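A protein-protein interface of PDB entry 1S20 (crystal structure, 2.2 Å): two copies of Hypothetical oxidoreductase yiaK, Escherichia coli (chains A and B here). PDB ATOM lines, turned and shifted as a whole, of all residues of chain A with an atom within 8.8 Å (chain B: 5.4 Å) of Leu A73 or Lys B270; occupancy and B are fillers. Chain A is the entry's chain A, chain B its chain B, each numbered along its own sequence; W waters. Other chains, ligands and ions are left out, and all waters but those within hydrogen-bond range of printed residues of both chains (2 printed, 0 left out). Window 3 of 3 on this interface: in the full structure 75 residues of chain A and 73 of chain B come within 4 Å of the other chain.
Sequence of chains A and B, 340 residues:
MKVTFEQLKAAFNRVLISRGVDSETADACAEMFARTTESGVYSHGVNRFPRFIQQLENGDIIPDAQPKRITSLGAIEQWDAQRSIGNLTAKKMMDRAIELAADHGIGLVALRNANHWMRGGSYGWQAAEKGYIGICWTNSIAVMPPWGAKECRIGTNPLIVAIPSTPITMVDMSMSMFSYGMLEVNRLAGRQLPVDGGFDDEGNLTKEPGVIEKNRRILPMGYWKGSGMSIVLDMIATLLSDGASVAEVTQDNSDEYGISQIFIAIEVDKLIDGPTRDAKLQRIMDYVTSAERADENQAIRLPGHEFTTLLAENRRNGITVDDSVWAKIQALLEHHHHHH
Water W1 bridges the backbone carbonyl oxygen of Leu B271 and the side-chain carboxylate of Asp A242. Water W2 lies within hydrogen-bond range of OE1 of Gln A78, OG1 of Thr A71 and O of Leu B271.
Leu A73 touches Gly B105. CD1 of Leu A73 touches CG of Glu B267, at 3.6 Å. Leu A73 touches Lys B270 (CD2 to O, 3.9 Å). His B104 touches Gly A74 (O to CA, 3.8 Å). CA of Gly B105 touches CG2 of Ile A76 (3.5 Å). CD1 of Ile A76 touches CD1 of Leu B271, 3.8 Å away. O of Leu A239 touches CB of Ile B272, at 3.8 Å. Leu A240 touches Glu B267. CB of Asp A242 touches O of Leu B271, 3.9 Å away. CG1 of Ile B272 touches OD1 of Asp A242, at 3.8 Å.
Of chain B, only His B104 (3.3 Å), Gly B105 (3.8 Å), Glu B267 (3.6 Å), Lys B270 (3.9 Å) and Leu B271 (3.5 Å) come within 4 Å of Leu A73. Printed residues of chain B within 4 Å of Gln A78: Leu B271. Of the printed residues of chain A, Gly B105 touches Leu A73 (3.8 Å) and Ile A76 (3.5 Å). Of the printed residues of chain B, Ile A76 touches His B104, Gly B105 and Leu B271. Of the printed residues of chain B, Asp A242 touches Leu B271 (3.9 Å) and Ile B272 (3.8 Å). Val B268 touches none of the printed residues of chain A. Leu A108 touches none of the printed residues of chain B. The nearest residue of chain B that does not touch Leu A73 is Asp B103 (4.3 Å). The nearest printed residue of chain B that does not touch Leu A240 is Val B268 (4.2 Å).
Printed residues of chain B that touch a printed residue of chain A: His B104, Gly B105, Glu B267, Lys B270, Leu B271 and Ile B272. Hydrophobic or aromatic side chains of chain B within 4 Å of the printed part of chain A: Leu B271 and Ile B272. Hydrophobic or aromatic side chains of chain A that line the printed part of chain B: Leu A73, Ala A75, Ile A76 and Leu A240. Among the printed residues, no Asp or Glu carboxylate lies within 4 Å of a Lys or Arg side-chain nitrogen of the other chain.
NE2 of Gln A78 sits at hydrogen-bond distance from O of Leu A240, at 3.0 Å. The side-chain amino group (NZ) of Lys B270 sits at hydrogen-bond distance from the backbone carbonyl oxygen (O) of Ala B102 (3.4 Å). N of Ile A70 is in hydrogen-bond range of O of Gln A78 (2.8 Å). OE2 of Glu B267 lies within hydrogen-bond range of N of Asp B269, 3.1 Å away. OE1 of Glu B267 is in salt-bridge range of NZ of Lys B270, at 3.9 Å. The backbone NH of Leu A108 is in hydrogen-bond range of the backbone carbonyl oxygen of Ala A75, at 3.0 Å.
The backbone carbonyl oxygen (O) of Leu A73 lies close to the backbone carbonyl oxygen (O) of His B104. N of Ala A75 sits at hydrogen-bond distance from O of His B104. NE2 of Gln A78 sits at hydrogen-bond distance from O of Leu B271 (3.0 Å).
Position printed for both chains: 104.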
ATOM      1  N   ARG A  69       4.656 -25.222   6.968  1.00  0.00           N
ATOM      2  CA  ARG A  69       5.534 -25.351   5.812  1.00  0.00           C
ATOM      3  C   ARG A  69       6.966 -25.510   6.290  1.00  0.00           C
ATOM      4  O   ARG A  69       7.369 -24.918   7.291  1.00  0.00           O
ATOM      5  CB  ARG A  69       5.452 -24.133   4.892  1.00  0.00           C
ATOM      6  CG  ARG A  69       6.077 -24.397   3.525  1.00  0.00           C
ATOM      7  CD  ARG A  69       6.996 -23.281   3.101  1.00  0.00           C
ATOM      8  NE  ARG A  69       6.275 -22.079   2.707  1.00  0.00           N
ATOM      9  CZ  ARG A  69       6.873 -20.931   2.416  1.00  0.00           C
ATOM     10  NH1 ARG A  69       8.194 -20.843   2.483  1.00  0.00           N
ATOM     11  NH2 ARG A  69       6.160 -19.876   2.046  1.00  0.00           N
ATOM     12  N   ILE A  70       7.734 -26.320   5.579  1.00  0.00           N
ATOM     13  CA  ILE A  70       9.117 -26.549   5.951  1.00  0.00           C
ATOM     14  C   ILE A  70      10.069 -25.883   4.960  1.00  0.00           C
ATOM     15  O   ILE A  70      10.774 -24.937   5.307  1.00  0.00           O
ATOM     16  CB  ILE A  70       9.432 -28.070   6.010  1.00  0.00           C
ATOM     17  CG1 ILE A  70       8.471 -28.777   6.975  1.00  0.00           C
ATOM     18  CG2 ILE A  70      10.873 -28.289   6.457  1.00  0.00           C
ATOM     19  CD1 ILE A  70       8.558 -28.292   8.412  1.00  0.00           C
ATOM     20  N   THR A  71      10.061 -26.371   3.724  1.00  0.00           N
ATOM     21  CA  THR A  71      10.948 -25.867   2.688  1.00  0.00           C
ATOM     22  C   THR A  71      10.218 -25.538   1.396  1.00  0.00           C
ATOM     23  O   THR A  71       9.217 -26.168   1.058  1.00  0.00           O
ATOM     24  CB  THR A  71      12.032 -26.914   2.377  1.00  0.00           C
ATOM     25  OG1 THR A  71      12.611 -27.366   3.608  1.00  0.00           O
ATOM     26  CG2 THR A  71      13.117 -26.332   1.487  1.00  0.00           C
ATOM     27  N   SER A  72      10.752 -24.562   0.671  1.00  0.00           N
ATOM     28  CA  SER A  72      10.183 -24.119  -0.591  1.00  0.00           C
ATOM     29  C   SER A  72      11.282 -23.944  -1.643  1.00  0.00           C
ATOM     30  O   SER A  72      12.227 -23.184  -1.448  1.00  0.00           O
ATOM     31  CB  SER A  72       9.445 -22.792  -0.387  1.00  0.00           C
ATOM     32  OG  SER A  72       9.093 -22.207  -1.625  1.00  0.00           O
ATOM     33  N   LEU A  73      11.151 -24.651  -2.759  1.00  0.00           N
ATOM     34  CA  LEU A  73      12.130 -24.571  -3.835  1.00  0.00           C
ATOM     35  C   LEU A  73      11.557 -23.772  -5.003  1.00  0.00           C
ATOM     36  O   LEU A  73      12.240 -23.529  -5.997  1.00  0.00           O
ATOM     37  CB  LEU A  73      12.507 -25.985  -4.308  1.00  0.00           C
ATOM     38  CG  LEU A  73      12.878 -27.001  -3.218  1.00  0.00           C
ATOM     39  CD1 LEU A  73      13.271 -28.342  -3.823  1.00  0.00           C
ATOM     40  CD2 LEU A  73      14.023 -26.440  -2.398  1.00  0.00           C
ATOM     41  N   GLY A  74      10.298 -23.361  -4.874  1.00  0.00           N
ATOM     42  CA  GLY A  74       9.646 -22.611  -5.934  1.00  0.00           C
ATOM     43  C   GLY A  74       8.276 -23.186  -6.246  1.00  0.00           C
ATOM     44  O   GLY A  74       7.291 -22.813  -5.605  1.00  0.00           O
ATOM     45  N   ALA A  75       8.207 -24.086  -7.228  1.00  0.00           N
ATOM     46  CA  ALA A  75       6.938 -24.715  -7.616  1.00  0.00           C
ATOM     47  C   ALA A  75       6.642 -25.955  -6.770  1.00  0.00           C
ATOM     48  O   ALA A  75       5.599 -26.602  -6.917  1.00  0.00           O
ATOM     49  CB  ALA A  75       6.966 -25.090  -9.101  1.00  0.00           C
ATOM     50  N   ILE A  76       7.569 -26.275  -5.875  1.00  0.00           N
ATOM     51  CA  ILE A  76       7.425 -27.430  -4.998  1.00  0.00           C
ATOM     52  C   ILE A  76       7.732 -27.012  -3.562  1.00  0.00           C
ATOM     53  O   ILE A  76       8.651 -26.220  -3.320  1.00  0.00           O
ATOM     54  CB  ILE A  76       8.391 -28.572  -5.429  1.00  0.00           C
ATOM     55  CG1 ILE A  76       8.151 -29.825  -4.576  1.00  0.00           C
ATOM     56  CG2 ILE A  76       9.833 -28.106  -5.302  1.00  0.00           C
ATOM     57  CD1 ILE A  76       8.923 -31.053  -5.048  1.00  0.00           C
ATOM     58  N   GLU A  77       6.942 -27.526  -2.622  1.00  0.00           N
ATOM     59  CA  GLU A  77       7.116 -27.228  -1.203  1.00  0.00           C
ATOM     60  C   GLU A  77       6.904 -28.479  -0.356  1.00  0.00           C
ATOM     61  O   GLU A  77       6.108 -29.358  -0.705  1.00  0.00           O
ATOM     62  CB  GLU A  77       6.122 -26.154  -0.726  1.00  0.00           C
ATOM     63  CG  GLU A  77       6.203 -24.793  -1.416  1.00  0.00           C
ATOM     64  CD  GLU A  77       5.226 -23.778  -0.822  1.00  0.00           C
ATOM     65  OE1 GLU A  77       4.119 -24.187  -0.410  1.00  0.00           O
ATOM     66  OE2 GLU A  77       5.564 -22.574  -0.769  1.00  0.00           O
ATOM     67  N   GLN A  78       7.614 -28.527   0.765  1.00  0.00           N
ATOM     68  CA  GLN A  78       7.538 -29.627   1.709  1.00  0.00           C
ATOM     69  C   GLN A  78       6.821 -29.125   2.959  1.00  0.00           C
ATOM     70  O   GLN A  78       7.280 -28.186   3.601  1.00  0.00           O
ATOM     71  CB  GLN A  78       8.948 -30.087   2.075  1.00  0.00           C
ATOM     72  CG  GLN A  78       9.001 -31.295   2.979  1.00  0.00           C
ATOM     73  CD  GLN A  78      10.427 -31.692   3.321  1.00  0.00           C
ATOM     74  OE1 GLN A  78      10.943 -31.350   4.390  1.00  0.00           O
ATOM     75  NE2 GLN A  78      11.075 -32.402   2.410  1.00  0.00           N
ATOM     76  N   ARG A  96      -2.877 -25.132  -1.688  1.00  0.00           N
ATOM     77  CA  ARG A  96      -1.555 -24.515  -1.735  1.00  0.00           C
ATOM     78  C   ARG A  96      -0.856 -24.902  -3.038  1.00  0.00           C
ATOM     79  O   ARG A  96      -0.049 -24.138  -3.573  1.00  0.00           O
ATOM     80  CB  ARG A  96      -0.700 -24.959  -0.537  1.00  0.00           C
ATOM     81  CG  ARG A  96       0.736 -24.428  -0.572  1.00  0.00           C
ATOM     82  CD  ARG A  96       0.777 -22.905  -0.529  1.00  0.00           C
ATOM     83  NE  ARG A  96       2.114 -22.374  -0.792  1.00  0.00           N
ATOM     84  CZ  ARG A  96       2.388 -21.083  -0.963  1.00  0.00           C
ATOM     85  NH1 ARG A  96       1.419 -20.181  -0.899  1.00  0.00           N
ATOM     86  NH2 ARG A  96       3.632 -20.694  -1.210  1.00  0.00           N
ATOM     87  N   LEU A 100       0.368 -22.466  -6.042  1.00  0.00           N
ATOM     88  CA  LEU A 100       1.693 -22.492  -6.652  1.00  0.00           C
ATOM     89  C   LEU A 100       1.613 -22.606  -8.178  1.00  0.00           C
ATOM     90  O   LEU A 100       2.343 -21.914  -8.896  1.00  0.00           O
ATOM     91  CB  LEU A 100       2.520 -23.650  -6.075  1.00  0.00           C
ATOM     92  CG  LEU A 100       2.995 -23.481  -4.625  1.00  0.00           C
ATOM     93  CD1 LEU A 100       3.618 -24.780  -4.120  1.00  0.00           C
ATOM     94  CD2 LEU A 100       4.005 -22.329  -4.547  1.00  0.00           C
ATOM     95  N   HIS A 104       3.401 -20.604 -11.196  1.00  0.00           N
ATOM     96  CA  HIS A 104       4.529 -21.355 -11.739  1.00  0.00           C
ATOM     97  C   HIS A 104       4.116 -22.365 -12.809  1.00  0.00           C
ATOM     98  O   HIS A 104       4.962 -23.053 -13.375  1.00  0.00           O
ATOM     99  CB  HIS A 104       5.274 -22.093 -10.622  1.00  0.00           C
ATOM    100  CG  HIS A 104       5.877 -21.189  -9.590  1.00  0.00           C
ATOM    101  ND1 HIS A 104       5.119 -20.496  -8.671  1.00  0.00           N
ATOM    102  CD2 HIS A 104       7.169 -20.883  -9.320  1.00  0.00           C
ATOM    103  CE1 HIS A 104       5.917 -19.804  -7.878  1.00  0.00           C
ATOM    104  NE2 HIS A 104       7.166 -20.022  -8.251  1.00  0.00           N
ATOM    105  N   LEU A 108       3.414 -28.554  -6.563  1.00  0.00           N
ATOM    106  CA  LEU A 108       3.467 -29.823  -5.867  1.00  0.00           C
ATOM    107  C   LEU A 108       3.733 -29.594  -4.396  1.00  0.00           C
ATOM    108  O   LEU A 108       4.588 -28.802  -4.027  1.00  0.00           O
ATOM    109  CB  LEU A 108       4.556 -30.720  -6.470  1.00  0.00           C
ATOM    110  CG  LEU A 108       4.575 -32.181  -6.009  1.00  0.00           C
ATOM    111  CD1 LEU A 108       5.299 -33.039  -7.026  1.00  0.00           C
ATOM    112  CD2 LEU A 108       5.236 -32.283  -4.646  1.00  0.00           C
ATOM    113  N   LEU A 239      10.249 -39.533   0.069  1.00  0.00           N
ATOM    114  CA  LEU A 239      11.382 -38.669  -0.247  1.00  0.00           C
ATOM    115  C   LEU A 239      11.069 -37.181  -0.244  1.00  0.00           C
ATOM    116  O   LEU A 239      11.674 -36.416   0.503  1.00  0.00           O
ATOM    117  CB  LEU A 239      11.949 -39.024  -1.620  1.00  0.00           C
ATOM    118  CG  LEU A 239      12.622 -40.375  -1.821  1.00  0.00           C
ATOM    119  CD1 LEU A 239      12.889 -40.562  -3.311  1.00  0.00           C
ATOM    120  CD2 LEU A 239      13.905 -40.457  -1.012  1.00  0.00           C
ATOM    121  N   LEU A 240      10.141 -36.773  -1.105  1.00  0.00           N
ATOM    122  CA  LEU A 240       9.772 -35.365  -1.225  1.00  0.00           C
ATOM    123  C   LEU A 240       9.254 -34.743   0.068  1.00  0.00           C
ATOM    124  O   LEU A 240       9.366 -33.537   0.271  1.00  0.00           O
ATOM    125  CB  LEU A 240       8.750 -35.195  -2.350  1.00  0.00           C
ATOM    126  CG  LEU A 240       9.304 -34.914  -3.753  1.00  0.00           C
ATOM    127  CD1 LEU A 240      10.604 -35.638  -3.989  1.00  0.00           C
ATOM    128  CD2 LEU A 240       8.264 -35.306  -4.780  1.00  0.00           C
ATOM    129  N   ASP A 242      10.149 -36.209   3.042  1.00  0.00           N
ATOM    130  CA  ASP A 242      11.129 -36.636   4.047  1.00  0.00           C
ATOM    131  C   ASP A 242      10.291 -37.139   5.209  1.00  0.00           C
ATOM    132  O   ASP A 242      10.502 -36.760   6.359  1.00  0.00           O
ATOM    133  CB  ASP A 242      12.000 -35.457   4.519  1.00  0.00           C
ATOM    134  CG  ASP A 242      13.232 -35.903   5.312  1.00  0.00           C
ATOM    135  OD1 ASP A 242      13.387 -37.112   5.594  1.00  0.00           O
ATOM    136  OD2 ASP A 242      14.055 -35.033   5.662  1.00  0.00           O
ATOM    137  N   ALA B 102      15.730 -28.003 -11.849  1.00  0.00           N
ATOM    138  CA  ALA B 102      16.919 -27.560 -11.130  1.00  0.00           C
ATOM    139  C   ALA B 102      16.749 -26.151 -10.557  1.00  0.00           C
ATOM    140  O   ALA B 102      17.286 -25.845  -9.496  1.00  0.00           O
ATOM    141  CB  ALA B 102      18.134 -27.611 -12.053  1.00  0.00           C
ATOM    142  N   ASP B 103      15.990 -25.302 -11.247  1.00  0.00           N
ATOM    143  CA  ASP B 103      15.781 -23.928 -10.791  1.00  0.00           C
ATOM    144  C   ASP B 103      14.385 -23.661 -10.220  1.00  0.00           C
ATOM    145  O   ASP B 103      14.111 -22.576  -9.705  1.00  0.00           O
ATOM    146  CB  ASP B 103      16.053 -22.963 -11.947  1.00  0.00           C
ATOM    147  CG  ASP B 103      17.409 -23.211 -12.602  1.00  0.00           C
ATOM    148  OD1 ASP B 103      18.440 -23.127 -11.895  1.00  0.00           O
ATOM    149  OD2 ASP B 103      17.442 -23.494 -13.823  1.00  0.00           O
ATOM    150  N   HIS B 104      13.511 -24.656 -10.305  1.00  0.00           N
ATOM    151  CA  HIS B 104      12.147 -24.519  -9.820  1.00  0.00           C
ATOM    152  C   HIS B 104      11.770 -25.608  -8.803  1.00  0.00           C
ATOM    153  O   HIS B 104      10.727 -25.524  -8.148  1.00  0.00           O
ATOM    154  CB  HIS B 104      11.186 -24.565 -11.009  1.00  0.00           C
ATOM    155  CG  HIS B 104      11.318 -23.404 -11.946  1.00  0.00           C
ATOM    156  ND1 HIS B 104      10.710 -22.188 -11.716  1.00  0.00           N
ATOM    157  CD2 HIS B 104      11.968 -23.280 -13.128  1.00  0.00           C
ATOM    158  CE1 HIS B 104      10.975 -21.368 -12.718  1.00  0.00           C
ATOM    159  NE2 HIS B 104      11.736 -22.007 -13.588  1.00  0.00           N
ATOM    160  N   GLY B 105      12.622 -26.621  -8.672  1.00  0.00           N
ATOM    161  CA  GLY B 105      12.347 -27.704  -7.741  1.00  0.00           C
ATOM    162  C   GLY B 105      11.615 -28.813  -8.461  1.00  0.00           C
ATOM    163  O   GLY B 105      11.711 -29.983  -8.107  1.00  0.00           O
ATOM    164  N   GLU B 267      13.156 -32.462  -8.143  1.00  0.00           N
ATOM    165  CA  GLU B 267      14.328 -32.338  -7.270  1.00  0.00           C
ATOM    166  C   GLU B 267      14.128 -33.194  -6.024  1.00  0.00           C
ATOM    167  O   GLU B 267      13.015 -33.311  -5.511  1.00  0.00           O
ATOM    168  CB  GLU B 267      14.521 -30.867  -6.852  1.00  0.00           C
ATOM    169  CG  GLU B 267      15.447 -30.628  -5.654  1.00  0.00           C
ATOM    170  CD  GLU B 267      16.917 -30.839  -5.978  1.00  0.00           C
ATOM    171  OE1 GLU B 267      17.377 -30.278  -6.991  1.00  0.00           O
ATOM    172  OE2 GLU B 267      17.611 -31.558  -5.221  1.00  0.00           O
ATOM    173  N   VAL B 268      15.210 -33.772  -5.526  1.00  0.00           N
ATOM    174  CA  VAL B 268      15.132 -34.615  -4.346  1.00  0.00           C
ATOM    175  C   VAL B 268      16.112 -34.211  -3.246  1.00  0.00           C
ATOM    176  O   VAL B 268      15.708 -33.928  -2.121  1.00  0.00           O
ATOM    177  CB  VAL B 268      15.401 -36.076  -4.721  1.00  0.00           C
ATOM    178  CG1 VAL B 268      15.371 -36.953  -3.474  1.00  0.00           C
ATOM    179  CG2 VAL B 268      14.372 -36.538  -5.734  1.00  0.00           C
ATOM    180  N   ASP B 269      17.399 -34.177  -3.583  1.00  0.00           N
ATOM    181  CA  ASP B 269      18.447 -33.852  -2.621  1.00  0.00           C
ATOM    182  C   ASP B 269      18.254 -32.561  -1.841  1.00  0.00           C
ATOM    183  O   ASP B 269      18.721 -32.456  -0.710  1.00  0.00           O
ATOM    184  CB  ASP B 269      19.814 -33.848  -3.315  1.00  0.00           C
ATOM    185  CG  ASP B 269      20.220 -35.232  -3.794  1.00  0.00           C
ATOM    186  OD1 ASP B 269      19.490 -36.200  -3.485  1.00  0.00           O
ATOM    187  OD2 ASP B 269      21.268 -35.359  -4.461  1.00  0.00           O
ATOM    188  N   LYS B 270      17.576 -31.580  -2.426  1.00  0.00           N
ATOM    189  CA  LYS B 270      17.346 -30.329  -1.711  1.00  0.00           C
ATOM    190  C   LYS B 270      16.106 -30.400  -0.826  1.00  0.00           C
ATOM    191  O   LYS B 270      15.621 -29.377  -0.348  1.00  0.00           O
ATOM    192  CB  LYS B 270      17.225 -29.151  -2.688  1.00  0.00           C
ATOM    193  CG  LYS B 270      18.573 -28.604  -3.120  1.00  0.00           C
ATOM    194  CD  LYS B 270      18.465 -27.372  -4.000  1.00  0.00           C
ATOM    195  CE  LYS B 270      18.260 -27.741  -5.462  1.00  0.00           C
ATOM    196  NZ  LYS B 270      18.273 -26.529  -6.337  1.00  0.00           N
ATOM    197  N   LEU B 271      15.599 -31.609  -0.598  1.00  0.00           N
ATOM    198  CA  LEU B 271      14.419 -31.802   0.246  1.00  0.00           C
ATOM    199  C   LEU B 271      14.693 -32.859   1.308  1.00  0.00           C
ATOM    200  O   LEU B 271      14.002 -32.926   2.324  1.00  0.00           O
ATOM    201  CB  LEU B 271      13.210 -32.234  -0.599  1.00  0.00           C
ATOM    202  CG  LEU B 271      12.733 -31.255  -1.672  1.00  0.00           C
ATOM    203  CD1 LEU B 271      11.666 -31.902  -2.555  1.00  0.00           C
ATOM    204  CD2 LEU B 271      12.187 -30.010  -0.986  1.00  0.00           C
ATOM    205  N   ILE B 272      15.719 -33.670   1.069  1.00  0.00           N
ATOM    206  CA  ILE B 272      16.088 -34.745   1.984  1.00  0.00           C
ATOM    207  C   ILE B 272      17.588 -35.046   1.897  1.00  0.00           C
ATOM    208  O   ILE B 272      18.135 -35.158   0.802  1.00  0.00           O
ATOM    209  CB  ILE B 272      15.313 -36.020   1.629  1.00  0.00           C
ATOM    210  CG1 ILE B 272      15.692 -37.145   2.597  1.00  0.00           C
ATOM    211  CG2 ILE B 272      15.597 -36.401   0.166  1.00  0.00           C
ATOM    212  CD1 ILE B 272      15.002 -38.459   2.313  1.00  0.00           C
HETATM  213  O   HOH W   1      14.415 -32.535   4.842  1.00  0.00           O
HETATM  214  O   HOH W   2      13.285 -30.073   3.984  1.00  0.00           O
